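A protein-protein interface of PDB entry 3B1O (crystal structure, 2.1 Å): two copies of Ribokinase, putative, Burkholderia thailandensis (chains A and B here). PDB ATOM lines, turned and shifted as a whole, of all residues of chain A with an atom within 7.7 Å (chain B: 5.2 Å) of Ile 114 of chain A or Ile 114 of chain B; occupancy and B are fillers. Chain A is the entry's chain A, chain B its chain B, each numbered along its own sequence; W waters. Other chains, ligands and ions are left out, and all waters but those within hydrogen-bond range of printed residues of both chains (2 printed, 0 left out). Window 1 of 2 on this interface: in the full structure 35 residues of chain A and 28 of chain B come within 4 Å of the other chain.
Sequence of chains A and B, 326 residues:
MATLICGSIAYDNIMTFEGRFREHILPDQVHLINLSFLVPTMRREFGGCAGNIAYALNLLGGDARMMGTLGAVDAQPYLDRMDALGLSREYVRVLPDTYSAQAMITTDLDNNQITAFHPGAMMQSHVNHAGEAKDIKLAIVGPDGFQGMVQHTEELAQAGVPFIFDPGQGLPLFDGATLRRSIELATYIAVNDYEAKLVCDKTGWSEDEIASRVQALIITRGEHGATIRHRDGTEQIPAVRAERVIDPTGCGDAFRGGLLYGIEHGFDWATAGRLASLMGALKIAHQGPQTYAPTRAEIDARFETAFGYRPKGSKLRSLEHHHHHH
The backbone carbonyl oxygen (O) of Leu 35 of chain A lies within hydrogen-bond range of the backbone NH (N) of Thr 115 of chain B (2.7 Å).
O of Ile 33 of chain B is in hydrogen-bond range of N of Gln 113 of chain A (2.6 Å).
SD of Met 15 of chain A sits close to SD of Met 104 of chain B, 3.5 Å away.
The backbone NH (N) of Phe 117 of chain A lies within hydrogen-bond range of the backbone carbonyl oxygen (O) of Phe 37 of chain B.
OD1 of Asn 112 of chain B lies within hydrogen-bond range of N of Ile 33 of chain A (2.7 Å).
The backbone NH (N) of Phe 37 of chain B lies within hydrogen-bond range of the backbone carbonyl oxygen (O) of Thr 115 of chain A (3.0 Å).
The side-chain amide oxygen (OD1) of Asn 112 of chain A is in hydrogen-bond range of the backbone NH (N) of Ile 33 of chain B (3.0 Å).
N of Leu 35 of chain A lies within hydrogen-bond range of O of Gln 113 of chain B, at 3.0 Å.
The backbone NH (N) of Gln 113 of chain B is in hydrogen-bond range of the backbone carbonyl oxygen (O) of Ile 33 of chain A (2.7 Å).
The backbone NH (N) of Phe 37 of chain A is in hydrogen-bond range of the backbone carbonyl oxygen (O) of Thr 115 of chain B (2.8 Å).
The backbone carbonyl oxygen of Gln 113 of chain A is in hydrogen-bond range of the backbone NH of Leu 35 of chain B (3.0 Å).
N of Phe 21 of chain A is in hydrogen-bond range of OD2 of Asp 108 of chain A (2.9 Å).
The side-chain hydroxyl (OG1) of Thr 107 of chain A is in hydrogen-bond range of the side-chain amide nitrogen (NE2) of Gln 113 of chain A.
Ile 114 of chain A touches just these residues of chain B: Leu 35 (3.4 Å), Phe 37 (3.9 Å) and Ile 114 (3.8 Å).
Ile 114 of chain B touches three residues of chain A.
Of the printed residues of chain B, Leu 35 of chain A touches Gln 113 (3.0 Å), Ile 114 (3.3 Å) and Thr 115 (2.7 Å).
Printed residues of chain B within 4 Å of Ser 36 of chain A: Thr 115.
The nearest residue of chain A that does not touch Ile 114 of chain B is Ile 25 of chain A (4.5 Å).
The nearest printed residue of chain A that does not touch Ala 116 of chain B is Met 15 of chain A (4.9 Å).
Printed residues of chain A that touch a printed residue of chain B: Met 15, Phe 21, Ile 33, Asn 34, Leu 35, Ser 36, Phe 37, Asn 112, Gln 113, Ile 114, Thr 115, Ala 116 and Phe 117.
Hydrophobic or aromatic side chains of chain A within 4 Å of the printed part of chain B: Met 15, Phe 21, Ile 33, Phe 37, Ile 114, Ala 116 and Phe 117.
Ile 33 of chain A touches Asn 112 of chain B, and with the chains exchanged Asn 112 of chain A touches Ile 33 of chain B.
Positions printed for both chains: 21, 33, 35, 37, 104, 105, 106, 107, 112, 113, 114, 115 and 116.
Water W1 lies within hydrogen-bond range of OG1 of Thr 115 of chain B (2.5 Å), OD1 of Asn 34 of chain A (3.0 Å) and O of Leu 35 of chain A (3.1 Å).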
ATOM      1  N   ASN A  13     -14.172   1.802 -21.362  1.00  0.00           N
ATOM      2  CA  ASN A  13     -14.237   1.996 -19.935  1.00  0.00           C
ATOM      3  C   ASN A  13     -13.088   1.210 -19.332  1.00  0.00           C
ATOM      4  O   ASN A  13     -13.163  -0.011 -19.172  1.00  0.00           O
ATOM      5  CB  ASN A  13     -15.592   1.554 -19.402  1.00  0.00           C
ATOM      6  CG  ASN A  13     -16.742   2.240 -20.113  1.00  0.00           C
ATOM      7  OD1 ASN A  13     -17.042   3.382 -19.836  1.00  0.00           O
ATOM      8  ND2 ASN A  13     -17.385   1.535 -21.051  1.00  0.00           N
ATOM      9  N   MET A  15     -10.318   0.102 -16.667  1.00  0.00           N
ATOM     10  CA  MET A  15     -10.158  -0.126 -15.239  1.00  0.00           C
ATOM     11  C   MET A  15      -8.784  -0.723 -14.998  1.00  0.00           C
ATOM     12  O   MET A  15      -8.225  -1.417 -15.861  1.00  0.00           O
ATOM     13  CB  MET A  15     -11.230  -1.090 -14.724  1.00  0.00           C
ATOM     14  CG  MET A  15     -12.650  -0.554 -14.846  1.00  0.00           C
ATOM     15  SD  MET A  15     -13.870  -1.872 -14.719  1.00  0.00           S
ATOM     16  CE  MET A  15     -13.865  -2.522 -16.386  1.00  0.00           C
ATOM     17  N   PHE A  17      -6.554  -3.191 -12.566  1.00  0.00           N
ATOM     18  CA  PHE A  17      -6.413  -4.173 -11.501  1.00  0.00           C
ATOM     19  C   PHE A  17      -5.011  -4.098 -10.911  1.00  0.00           C
ATOM     20  O   PHE A  17      -4.011  -4.372 -11.592  1.00  0.00           O
ATOM     21  CB  PHE A  17      -6.702  -5.590 -12.025  1.00  0.00           C
ATOM     22  CG  PHE A  17      -6.392  -6.693 -11.037  1.00  0.00           C
ATOM     23  CD1 PHE A  17      -6.665  -6.544  -9.681  1.00  0.00           C
ATOM     24  CD2 PHE A  17      -5.863  -7.904 -11.481  1.00  0.00           C
ATOM     25  CE1 PHE A  17      -6.389  -7.569  -8.778  1.00  0.00           C
ATOM     26  CE2 PHE A  17      -5.595  -8.941 -10.590  1.00  0.00           C
ATOM     27  CZ  PHE A  17      -5.859  -8.774  -9.236  1.00  0.00           C
ATOM     28  N   PHE A  21      -3.487 -11.014 -13.270  1.00  0.00           N
ATOM     29  CA  PHE A  21      -4.389 -12.089 -13.664  1.00  0.00           C
ATOM     30  C   PHE A  21      -3.667 -13.434 -13.654  1.00  0.00           C
ATOM     31  O   PHE A  21      -4.259 -14.446 -13.292  1.00  0.00           O
ATOM     32  CB  PHE A  21      -4.990 -11.839 -15.047  1.00  0.00           C
ATOM     33  CG  PHE A  21      -5.951 -10.682 -15.100  1.00  0.00           C
ATOM     34  CD1 PHE A  21      -7.038 -10.613 -14.226  1.00  0.00           C
ATOM     35  CD2 PHE A  21      -5.793  -9.680 -16.060  1.00  0.00           C
ATOM     36  CE1 PHE A  21      -7.934  -9.552 -14.292  1.00  0.00           C
ATOM     37  CE2 PHE A  21      -6.677  -8.617 -16.134  1.00  0.00           C
ATOM     38  CZ  PHE A  21      -7.752  -8.549 -15.252  1.00  0.00           C
ATOM     39  N   HIS A  24      -3.955 -15.628 -10.626  1.00  0.00           N
ATOM     40  CA  HIS A  24      -5.251 -16.183 -10.235  1.00  0.00           C
ATOM     41  C   HIS A  24      -5.895 -17.063 -11.308  1.00  0.00           C
ATOM     42  O   HIS A  24      -6.766 -17.883 -10.991  1.00  0.00           O
ATOM     43  CB  HIS A  24      -6.222 -15.061  -9.873  1.00  0.00           C
ATOM     44  CG  HIS A  24      -5.643 -14.018  -8.973  1.00  0.00           C
ATOM     45  ND1 HIS A  24      -5.760 -14.071  -7.602  1.00  0.00           N
ATOM     46  CD2 HIS A  24      -4.946 -12.891  -9.247  1.00  0.00           C
ATOM     47  CE1 HIS A  24      -5.153 -13.025  -7.070  1.00  0.00           C
ATOM     48  NE2 HIS A  24      -4.661 -12.288  -8.048  1.00  0.00           N
ATOM     49  N   ILE A  25      -5.487 -16.866 -12.566  1.00  0.00           N
ATOM     50  CA  ILE A  25      -6.015 -17.648 -13.696  1.00  0.00           C
ATOM     51  C   ILE A  25      -4.916 -18.531 -14.306  1.00  0.00           C
ATOM     52  O   ILE A  25      -4.170 -18.084 -15.169  1.00  0.00           O
ATOM     53  CB  ILE A  25      -6.635 -16.751 -14.822  1.00  0.00           C
ATOM     54  CG1 ILE A  25      -7.436 -15.557 -14.262  1.00  0.00           C
ATOM     55  CG2 ILE A  25      -7.469 -17.582 -15.775  1.00  0.00           C
ATOM     56  CD1 ILE A  25      -8.629 -15.911 -13.415  1.00  0.00           C
ATOM     57  N   ILE A  33     -12.531 -20.358  -9.987  1.00  0.00           N
ATOM     58  CA  ILE A  33     -11.939 -19.039  -9.795  1.00  0.00           C
ATOM     59  C   ILE A  33     -12.963 -18.068  -9.210  1.00  0.00           C
ATOM     60  O   ILE A  33     -14.124 -18.025  -9.619  1.00  0.00           O
ATOM     61  CB  ILE A  33     -11.315 -18.472 -11.088  1.00  0.00           C
ATOM     62  CG1 ILE A  33     -10.206 -19.409 -11.592  1.00  0.00           C
ATOM     63  CG2 ILE A  33     -10.748 -17.085 -10.828  1.00  0.00           C
ATOM     64  CD1 ILE A  33      -9.895 -19.270 -13.079  1.00  0.00           C
ATOM     65  N   ASN A  34     -12.506 -17.333  -8.211  1.00  0.00           N
ATOM     66  CA  ASN A  34     -13.291 -16.319  -7.544  1.00  0.00           C
ATOM     67  C   ASN A  34     -12.393 -15.099  -7.342  1.00  0.00           C
ATOM     68  O   ASN A  34     -12.072 -14.759  -6.221  1.00  0.00           O
ATOM     69  CB  ASN A  34     -13.764 -16.874  -6.199  1.00  0.00           C
ATOM     70  CG  ASN A  34     -15.018 -16.190  -5.683  1.00  0.00           C
ATOM     71  OD1 ASN A  34     -15.331 -15.048  -6.043  1.00  0.00           O
ATOM     72  ND2 ASN A  34     -15.744 -16.892  -4.817  1.00  0.00           N
ATOM     73  N   LEU A  35     -11.947 -14.479  -8.435  1.00  0.00           N
ATOM     74  CA  LEU A  35     -11.092 -13.303  -8.364  1.00  0.00           C
ATOM     75  C   LEU A  35     -11.972 -12.100  -8.035  1.00  0.00           C
ATOM     76  O   LEU A  35     -12.844 -11.716  -8.828  1.00  0.00           O
ATOM     77  CB  LEU A  35     -10.390 -13.058  -9.709  1.00  0.00           C
ATOM     78  CG  LEU A  35      -9.026 -12.341  -9.849  1.00  0.00           C
ATOM     79  CD1 LEU A  35      -8.896 -11.689 -11.187  1.00  0.00           C
ATOM     80  CD2 LEU A  35      -8.691 -11.328  -8.756  1.00  0.00           C
ATOM     81  N   SER A  36     -11.736 -11.496  -6.880  1.00  0.00           N
ATOM     82  CA  SER A  36     -12.513 -10.344  -6.460  1.00  0.00           C
ATOM     83  C   SER A  36     -11.565  -9.179  -6.160  1.00  0.00           C
ATOM     84  O   SER A  36     -10.649  -9.319  -5.354  1.00  0.00           O
ATOM     85  CB  SER A  36     -13.343 -10.717  -5.226  1.00  0.00           C
ATOM     86  OG  SER A  36     -14.366  -9.772  -4.991  1.00  0.00           O
ATOM     87  N   PHE A  37     -11.769  -8.037  -6.814  1.00  0.00           N
ATOM     88  CA  PHE A  37     -10.887  -6.884  -6.602  1.00  0.00           C
ATOM     89  C   PHE A  37     -11.564  -5.511  -6.722  1.00  0.00           C
ATOM     90  O   PHE A  37     -12.645  -5.378  -7.311  1.00  0.00           O
ATOM     91  CB  PHE A  37      -9.650  -6.960  -7.508  1.00  0.00           C
ATOM     92  CG  PHE A  37      -9.962  -6.984  -8.981  1.00  0.00           C
ATOM     93  CD1 PHE A  37     -10.099  -8.199  -9.652  1.00  0.00           C
ATOM     94  CD2 PHE A  37     -10.089  -5.800  -9.706  1.00  0.00           C
ATOM     95  CE1 PHE A  37     -10.382  -8.238 -11.022  1.00  0.00           C
ATOM     96  CE2 PHE A  37     -10.362  -5.822 -11.076  1.00  0.00           C
ATOM     97  CZ  PHE A  37     -10.513  -7.040 -11.745  1.00  0.00           C
ATOM     98  N   ALA A 103     -16.799  -1.048 -24.254  1.00  0.00           N
ATOM     99  CA  ALA A 103     -15.739  -1.969 -23.822  1.00  0.00           C
ATOM    100  C   ALA A 103     -15.466  -1.810 -22.330  1.00  0.00           C
ATOM    101  O   ALA A 103     -15.076  -0.728 -21.904  1.00  0.00           O
ATOM    102  CB  ALA A 103     -14.470  -1.672 -24.596  1.00  0.00           C
ATOM    103  N   MET A 104     -15.663  -2.874 -21.547  1.00  0.00           N
ATOM    104  CA  MET A 104     -15.260  -2.903 -20.123  1.00  0.00           C
ATOM    105  C   MET A 104     -13.879  -3.538 -20.001  1.00  0.00           C
ATOM    106  O   MET A 104     -13.757  -4.767 -19.872  1.00  0.00           O
ATOM    107  CB  MET A 104     -16.250  -3.696 -19.248  1.00  0.00           C
ATOM    108  CG  MET A 104     -17.733  -3.459 -19.512  1.00  0.00           C
ATOM    109  SD  MET A 104     -18.118  -1.723 -19.719  1.00  0.00           S
ATOM    110  CE  MET A 104     -17.765  -1.125 -18.049  1.00  0.00           C
ATOM    111  N   ILE A 105     -12.850  -2.695 -20.036  1.00  0.00           N
ATOM    112  CA  ILE A 105     -11.460  -3.137 -20.144  1.00  0.00           C
ATOM    113  C   ILE A 105     -10.774  -3.117 -18.796  1.00  0.00           C
ATOM    114  O   ILE A 105     -10.699  -2.078 -18.152  1.00  0.00           O
ATOM    115  CB  ILE A 105     -10.649  -2.239 -21.122  1.00  0.00           C
ATOM    116  CG1 ILE A 105     -11.361  -2.118 -22.467  1.00  0.00           C
ATOM    117  CG2 ILE A 105      -9.237  -2.803 -21.339  1.00  0.00           C
ATOM    118  CD1 ILE A 105     -10.802  -1.047 -23.393  1.00  0.00           C
ATOM    119  N   THR A 106     -10.264  -4.266 -18.363  1.00  0.00           N
ATOM    120  CA  THR A 106      -9.482  -4.316 -17.130  1.00  0.00           C
ATOM    121  C   THR A 106      -8.036  -4.634 -17.469  1.00  0.00           C
ATOM    122  O   THR A 106      -7.747  -5.605 -18.181  1.00  0.00           O
ATOM    123  CB  THR A 106     -10.007  -5.341 -16.115  1.00  0.00           C
ATOM    124  OG1 THR A 106     -11.412  -5.162 -15.913  1.00  0.00           O
ATOM    125  CG2 THR A 106      -9.295  -5.171 -14.770  1.00  0.00           C
ATOM    126  N   THR A 107      -7.137  -3.813 -16.941  1.00  0.00           N
ATOM    127  CA  THR A 107      -5.718  -3.922 -17.224  1.00  0.00           C
ATOM    128  C   THR A 107      -5.016  -4.232 -15.914  1.00  0.00           C
ATOM    129  O   THR A 107      -5.332  -3.643 -14.879  1.00  0.00           O
ATOM    130  CB  THR A 107      -5.187  -2.614 -17.877  1.00  0.00           C
ATOM    131  OG1 THR A 107      -5.952  -2.339 -19.055  1.00  0.00           O
ATOM    132  CG2 THR A 107      -3.716  -2.725 -18.255  1.00  0.00           C
ATOM    133  N   ASP A 108      -4.100  -5.190 -15.947  1.00  0.00           N
ATOM    134  CA  ASP A 108      -3.344  -5.540 -14.747  1.00  0.00           C
ATOM    135  C   ASP A 108      -1.897  -5.029 -14.851  1.00  0.00           C
ATOM    136  O   ASP A 108      -1.505  -4.483 -15.902  1.00  0.00           O
ATOM    137  CB  ASP A 108      -3.424  -7.049 -14.475  1.00  0.00           C
ATOM    138  CG  ASP A 108      -2.511  -7.873 -15.375  1.00  0.00           C
ATOM    139  OD1 ASP A 108      -1.753  -7.303 -16.184  1.00  0.00           O
ATOM    140  OD2 ASP A 108      -2.544  -9.119 -15.267  1.00  0.00           O
ATOM    141  N   ASN A 111       0.272  -5.385 -17.863  1.00  0.00           N
ATOM    142  CA  ASN A 111      -0.386  -4.889 -19.074  1.00  0.00           C
ATOM    143  C   ASN A 111      -1.188  -5.968 -19.795  1.00  0.00           C
ATOM    144  O   ASN A 111      -1.443  -5.885 -21.003  1.00  0.00           O
ATOM    145  CB  ASN A 111       0.603  -4.188 -20.001  1.00  0.00           C
ATOM    146  CG  ASN A 111       1.152  -2.928 -19.391  1.00  0.00           C
ATOM    147  OD1 ASN A 111       2.337  -2.853 -19.070  1.00  0.00           O
ATOM    148  ND2 ASN A 111       0.284  -1.937 -19.187  1.00  0.00           N
ATOM    149  N   ASN A 112      -1.589  -6.982 -19.030  1.00  0.00           N
ATOM    150  CA  ASN A 112      -2.519  -7.991 -19.515  1.00  0.00           C
ATOM    151  C   ASN A 112      -3.930  -7.438 -19.405  1.00  0.00           C
ATOM    152  O   ASN A 112      -4.208  -6.634 -18.518  1.00  0.00           O
ATOM    153  CB  ASN A 112      -2.361  -9.287 -18.702  1.00  0.00           C
ATOM    154  CG  ASN A 112      -1.140 -10.084 -19.115  1.00  0.00           C
ATOM    155  OD1 ASN A 112      -0.792 -10.128 -20.300  1.00  0.00           O
ATOM    156  ND2 ASN A 112      -0.494 -10.736 -18.151  1.00  0.00           N
ATOM    157  N   GLN A 113      -4.814  -7.855 -20.304  1.00  0.00           N
ATOM    158  CA  GLN A 113      -6.169  -7.297 -20.358  1.00  0.00           C
ATOM    159  C   GLN A 113      -7.279  -8.326 -20.508  1.00  0.00           C
ATOM    160  O   GLN A 113      -7.118  -9.353 -21.189  1.00  0.00           O
ATOM    161  CB  GLN A 113      -6.280  -6.261 -21.490  1.00  0.00           C
ATOM    162  CG  GLN A 113      -5.442  -5.007 -21.254  1.00  0.00           C
ATOM    163  CD  GLN A 113      -5.749  -3.910 -22.245  1.00  0.00           C
ATOM    164  OE1 GLN A 113      -5.939  -4.163 -23.439  1.00  0.00           O
ATOM    165  NE2 GLN A 113      -5.800  -2.679 -21.754  1.00  0.00           N
ATOM    166  N   ILE A 114      -8.405  -8.040 -19.860  1.00  0.00           N
ATOM    167  CA  ILE A 114      -9.641  -8.771 -20.089  1.00  0.00           C
ATOM    168  C   ILE A 114     -10.744  -7.752 -20.404  1.00  0.00           C
ATOM    169  O   ILE A 114     -11.031  -6.853 -19.603  1.00  0.00           O
ATOM    170  CB  ILE A 114     -10.022  -9.662 -18.872  1.00  0.00           C
ATOM    171  CG1 ILE A 114      -8.896 -10.665 -18.573  1.00  0.00           C
ATOM    172  CG2 ILE A 114     -11.373 -10.365 -19.105  1.00  0.00           C
ATOM    173  CD1 ILE A 114      -9.192 -11.630 -17.430  1.00  0.00           C
ATOM    174  N   THR A 115     -11.350  -7.911 -21.569  1.00  0.00           N
ATOM    175  CA  THR A 115     -12.401  -7.024 -22.050  1.00  0.00           C
ATOM    176  C   THR A 115     -13.768  -7.721 -22.179  1.00  0.00           C
ATOM    177  O   THR A 115     -13.888  -8.730 -22.869  1.00  0.00           O
ATOM    178  CB  THR A 115     -11.997  -6.395 -23.403  1.00  0.00           C
ATOM    179  OG1 THR A 115     -10.760  -5.691 -23.241  1.00  0.00           O
ATOM    180  CG2 THR A 115     -13.069  -5.411 -23.903  1.00  0.00           C
ATOM    181  N   ALA A 116     -14.779  -7.193 -21.490  1.00  0.00           N
ATOM    182  CA  ALA A 116     -16.169  -7.522 -21.810  1.00  0.00           C
ATOM    183  C   ALA A 116     -16.716  -6.454 -22.752  1.00  0.00           C
ATOM    184  O   ALA A 116     -16.824  -5.271 -22.392  1.00  0.00           O
ATOM    185  CB  ALA A 116     -17.024  -7.615 -20.571  1.00  0.00           C
ATOM    186  N   PHE A 117     -17.069  -6.886 -23.955  1.00  0.00           N
ATOM    187  CA  PHE A 117     -17.502  -5.975 -25.018  1.00  0.00           C
ATOM    188  C   PHE A 117     -19.029  -6.020 -25.216  1.00  0.00           C
ATOM    189  O   PHE A 117     -19.584  -7.023 -25.707  1.00  0.00           O
ATOM    190  CB  PHE A 117     -16.761  -6.287 -26.316  1.00  0.00           C
ATOM    191  CG  PHE A 117     -16.799  -5.165 -27.304  1.00  0.00           C
ATOM    192  CD1 PHE A 117     -15.819  -4.185 -27.290  1.00  0.00           C
ATOM    193  CD2 PHE A 117     -17.850  -5.068 -28.216  1.00  0.00           C
ATOM    194  CE1 PHE A 117     -15.869  -3.112 -28.189  1.00  0.00           C
ATOM    195  CE2 PHE A 117     -17.915  -4.012 -29.120  1.00  0.00           C
ATOM    196  CZ  PHE A 117     -16.923  -3.024 -29.104  1.00  0.00           C
ATOM    197  N   PHE B  21     -12.252 -18.978 -19.133  1.00  0.00           N
ATOM    198  CA  PHE B  21     -11.144 -18.080 -18.815  1.00  0.00           C
ATOM    199  C   PHE B  21      -9.789 -18.755 -19.013  1.00  0.00           C
ATOM    200  O   PHE B  21      -8.873 -18.159 -19.588  1.00  0.00           O
ATOM    201  CB  PHE B  21     -11.234 -17.539 -17.377  1.00  0.00           C
ATOM    202  CG  PHE B  21     -12.364 -16.552 -17.146  1.00  0.00           C
ATOM    203  CD1 PHE B  21     -13.167 -16.667 -16.023  1.00  0.00           C
ATOM    204  CD2 PHE B  21     -12.603 -15.503 -18.037  1.00  0.00           C
ATOM    205  CE1 PHE B  21     -14.206 -15.763 -15.782  1.00  0.00           C
ATOM    206  CE2 PHE B  21     -13.646 -14.599 -17.815  1.00  0.00           C
ATOM    207  CZ  PHE B  21     -14.450 -14.740 -16.669  1.00  0.00           C
ATOM    208  N   ILE B  33      -2.531 -12.398 -21.172  1.00  0.00           N
ATOM    209  CA  ILE B  33      -3.961 -12.501 -21.434  1.00  0.00           C
ATOM    210  C   ILE B  33      -4.468 -11.185 -22.032  1.00  0.00           C
ATOM    211  O   ILE B  33      -4.224 -10.101 -21.490  1.00  0.00           O
ATOM    212  CB  ILE B  33      -4.805 -13.040 -20.221  1.00  0.00           C
ATOM    213  CG1 ILE B  33      -6.290 -13.134 -20.589  1.00  0.00           C
ATOM    214  CG2 ILE B  33      -4.595 -12.220 -18.967  1.00  0.00           C
ATOM    215  CD1 ILE B  33      -6.965 -14.380 -20.083  1.00  0.00           C
ATOM    216  N   LEU B  35      -7.921 -10.953 -23.583  1.00  0.00           N
ATOM    217  CA  LEU B  35      -9.170 -11.584 -23.927  1.00  0.00           C
ATOM    218  C   LEU B  35     -10.216 -10.510 -24.125  1.00  0.00           C
ATOM    219  O   LEU B  35     -10.377  -9.632 -23.280  1.00  0.00           O
ATOM    220  CB  LEU B  35      -9.582 -12.529 -22.798  1.00  0.00           C
ATOM    221  CG  LEU B  35     -10.957 -13.215 -22.802  1.00  0.00           C
ATOM    222  CD1 LEU B  35     -11.128 -14.131 -24.024  1.00  0.00           C
ATOM    223  CD2 LEU B  35     -11.141 -13.996 -21.480  1.00  0.00           C
ATOM    224  N   PHE B  37     -14.430 -10.591 -25.219  1.00  0.00           N
ATOM    225  CA  PHE B  37     -15.581 -11.411 -25.554  1.00  0.00           C
ATOM    226  C   PHE B  37     -16.853 -10.566 -25.580  1.00  0.00           C
ATOM    227  O   PHE B  37     -16.990  -9.583 -24.836  1.00  0.00           O
ATOM    228  CB  PHE B  37     -15.719 -12.579 -24.567  1.00  0.00           C
ATOM    229  CG  PHE B  37     -15.684 -12.158 -23.121  1.00  0.00           C
ATOM    230  CD1 PHE B  37     -14.475 -12.123 -22.420  1.00  0.00           C
ATOM    231  CD2 PHE B  37     -16.851 -11.792 -22.462  1.00  0.00           C
ATOM    232  CE1 PHE B  37     -14.421 -11.720 -21.086  1.00  0.00           C
ATOM    233  CE2 PHE B  37     -16.815 -11.382 -21.109  1.00  0.00           C
ATOM    234  CZ  PHE B  37     -15.584 -11.346 -20.427  1.00  0.00           C
ATOM    235  N   MET B 104     -18.826  -5.219 -11.465  1.00  0.00           N
ATOM    236  CA  MET B 104     -18.803  -6.010 -12.688  1.00  0.00           C
ATOM    237  C   MET B 104     -18.509  -7.465 -12.356  1.00  0.00           C
ATOM    238  O   MET B 104     -17.486  -7.782 -11.743  1.00  0.00           O
ATOM    239  CB  MET B 104     -17.780  -5.446 -13.660  1.00  0.00           C
ATOM    240  CG  MET B 104     -18.339  -4.296 -14.457  1.00  0.00           C
ATOM    241  SD  MET B 104     -17.215  -2.930 -14.364  1.00  0.00           S
ATOM    242  CE  MET B 104     -17.606  -2.222 -12.763  1.00  0.00           C
ATOM    243  N   ILE B 105     -19.434  -8.334 -12.732  1.00  0.00           N
ATOM    244  CA  ILE B 105     -19.380  -9.742 -12.369  1.00  0.00           C
ATOM    245  C   ILE B 105     -19.471 -10.600 -13.620  1.00  0.00           C
ATOM    246  O   ILE B 105     -20.499 -10.632 -14.305  1.00  0.00           O
ATOM    247  CB  ILE B 105     -20.494 -10.111 -11.362  1.00  0.00           C
ATOM    248  CG1 ILE B 105     -20.392  -9.220 -10.120  1.00  0.00           C
ATOM    249  CG2 ILE B 105     -20.394 -11.582 -10.968  1.00  0.00           C
ATOM    250  CD1 ILE B 105     -21.737  -8.828  -9.496  1.00  0.00           C
ATOM    251  N   THR B 106     -18.373 -11.284 -13.915  1.00  0.00           N
ATOM    252  CA  THR B 106     -18.278 -12.094 -15.119  1.00  0.00           C
ATOM    253  C   THR B 106     -18.084 -13.541 -14.743  1.00  0.00           C
ATOM    254  O   THR B 106     -17.146 -13.879 -14.023  1.00  0.00           O
ATOM    255  CB  THR B 106     -17.118 -11.637 -16.035  1.00  0.00           C
ATOM    256  OG1 THR B 106     -17.211 -10.233 -16.261  1.00  0.00           O
ATOM    257  CG2 THR B 106     -17.174 -12.346 -17.378  1.00  0.00           C
ATOM    258  N   THR B 107     -18.973 -14.398 -15.229  1.00  0.00           N
ATOM    259  CA  THR B 107     -18.807 -15.830 -15.021  1.00  0.00           C
ATOM    260  C   THR B 107     -18.660 -16.550 -16.356  1.00  0.00           C
ATOM    261  O   THR B 107     -19.341 -16.218 -17.343  1.00  0.00           O
ATOM    262  CB  THR B 107     -19.941 -16.450 -14.144  1.00  0.00           C
ATOM    263  OG1 THR B 107     -20.972 -16.979 -14.975  1.00  0.00           O
ATOM    264  CG2 THR B 107     -20.543 -15.409 -13.218  1.00  0.00           C
ATOM    265  N   ASN B 112     -16.384 -20.143 -13.118  1.00  0.00           N
ATOM    266  CA  ASN B 112     -15.311 -19.276 -12.623  1.00  0.00           C
ATOM    267  C   ASN B 112     -15.793 -17.832 -12.696  1.00  0.00           C
ATOM    268  O   ASN B 112     -16.407 -17.456 -13.695  1.00  0.00           O
ATOM    269  CB  ASN B 112     -14.067 -19.412 -13.504  1.00  0.00           C
ATOM    270  CG  ASN B 112     -13.506 -20.811 -13.521  1.00  0.00           C
ATOM    271  OD1 ASN B 112     -13.058 -21.314 -12.502  1.00  0.00           O
ATOM    272  ND2 ASN B 112     -13.500 -21.439 -14.702  1.00  0.00           N
ATOM    273  N   GLN B 113     -15.526 -17.039 -11.657  1.00  0.00           N
ATOM    274  CA  GLN B 113     -15.987 -15.644 -11.590  1.00  0.00           C
ATOM    275  C   GLN B 113     -14.861 -14.651 -11.399  1.00  0.00           C
ATOM    276  O   GLN B 113     -13.876 -14.940 -10.720  1.00  0.00           O
ATOM    277  CB  GLN B 113     -16.964 -15.415 -10.430  1.00  0.00           C
ATOM    278  CG  GLN B 113     -18.269 -16.140 -10.516  1.00  0.00           C
ATOM    279  CD  GLN B 113     -19.326 -15.517  -9.618  1.00  0.00           C
ATOM    280  OE1 GLN B 113     -19.016 -14.852  -8.627  1.00  0.00           O
ATOM    281  NE2 GLN B 113     -20.587 -15.723  -9.973  1.00  0.00           N
ATOM    282  N   ILE B 114     -15.047 -13.473 -11.991  1.00  0.00           N
ATOM    283  CA  ILE B 114     -14.205 -12.304 -11.769  1.00  0.00           C
ATOM    284  C   ILE B 114     -15.119 -11.139 -11.382  1.00  0.00           C
ATOM    285  O   ILE B 114     -16.018 -10.767 -12.149  1.00  0.00           O
ATOM    286  CB  ILE B 114     -13.375 -11.908 -13.019  1.00  0.00           C
ATOM    287  CG1 ILE B 114     -12.451 -13.056 -13.464  1.00  0.00           C
ATOM    288  CG2 ILE B 114     -12.574 -10.630 -12.736  1.00  0.00           C
ATOM    289  CD1 ILE B 114     -11.658 -12.800 -14.734  1.00  0.00           C
ATOM    290  N   THR B 115     -14.877 -10.568 -10.206  1.00  0.00           N
ATOM    291  CA  THR B 115     -15.686  -9.455  -9.679  1.00  0.00           C
ATOM    292  C   THR B 115     -14.838  -8.197  -9.468  1.00  0.00           C
ATOM    293  O   THR B 115     -13.919  -8.195  -8.654  1.00  0.00           O
ATOM    294  CB  THR B 115     -16.362  -9.827  -8.322  1.00  0.00           C
ATOM    295  OG1 THR B 115     -17.139 -11.026  -8.468  1.00  0.00           O
ATOM    296  CG2 THR B 115     -17.264  -8.696  -7.819  1.00  0.00           C
ATOM    297  N   ALA B 116     -15.142  -7.133 -10.200  1.00  0.00           N
ATOM    298  CA  ALA B 116     -14.487  -5.853  -9.954  1.00  0.00           C
ATOM    299  C   ALA B 116     -15.523  -4.867  -9.460  1.00  0.00           C
ATOM    300  O   ALA B 116     -16.549  -4.668 -10.112  1.00  0.00           O
ATOM    301  CB  ALA B 116     -13.810  -5.334 -11.209  1.00  0.00           C
HETATM  302  O   HOH W   1     -15.570 -12.950  -8.161  1.00  0.00           O
HETATM  303  O   HOH W   2     -15.123  -6.894  -6.001  1.00  0.00           O
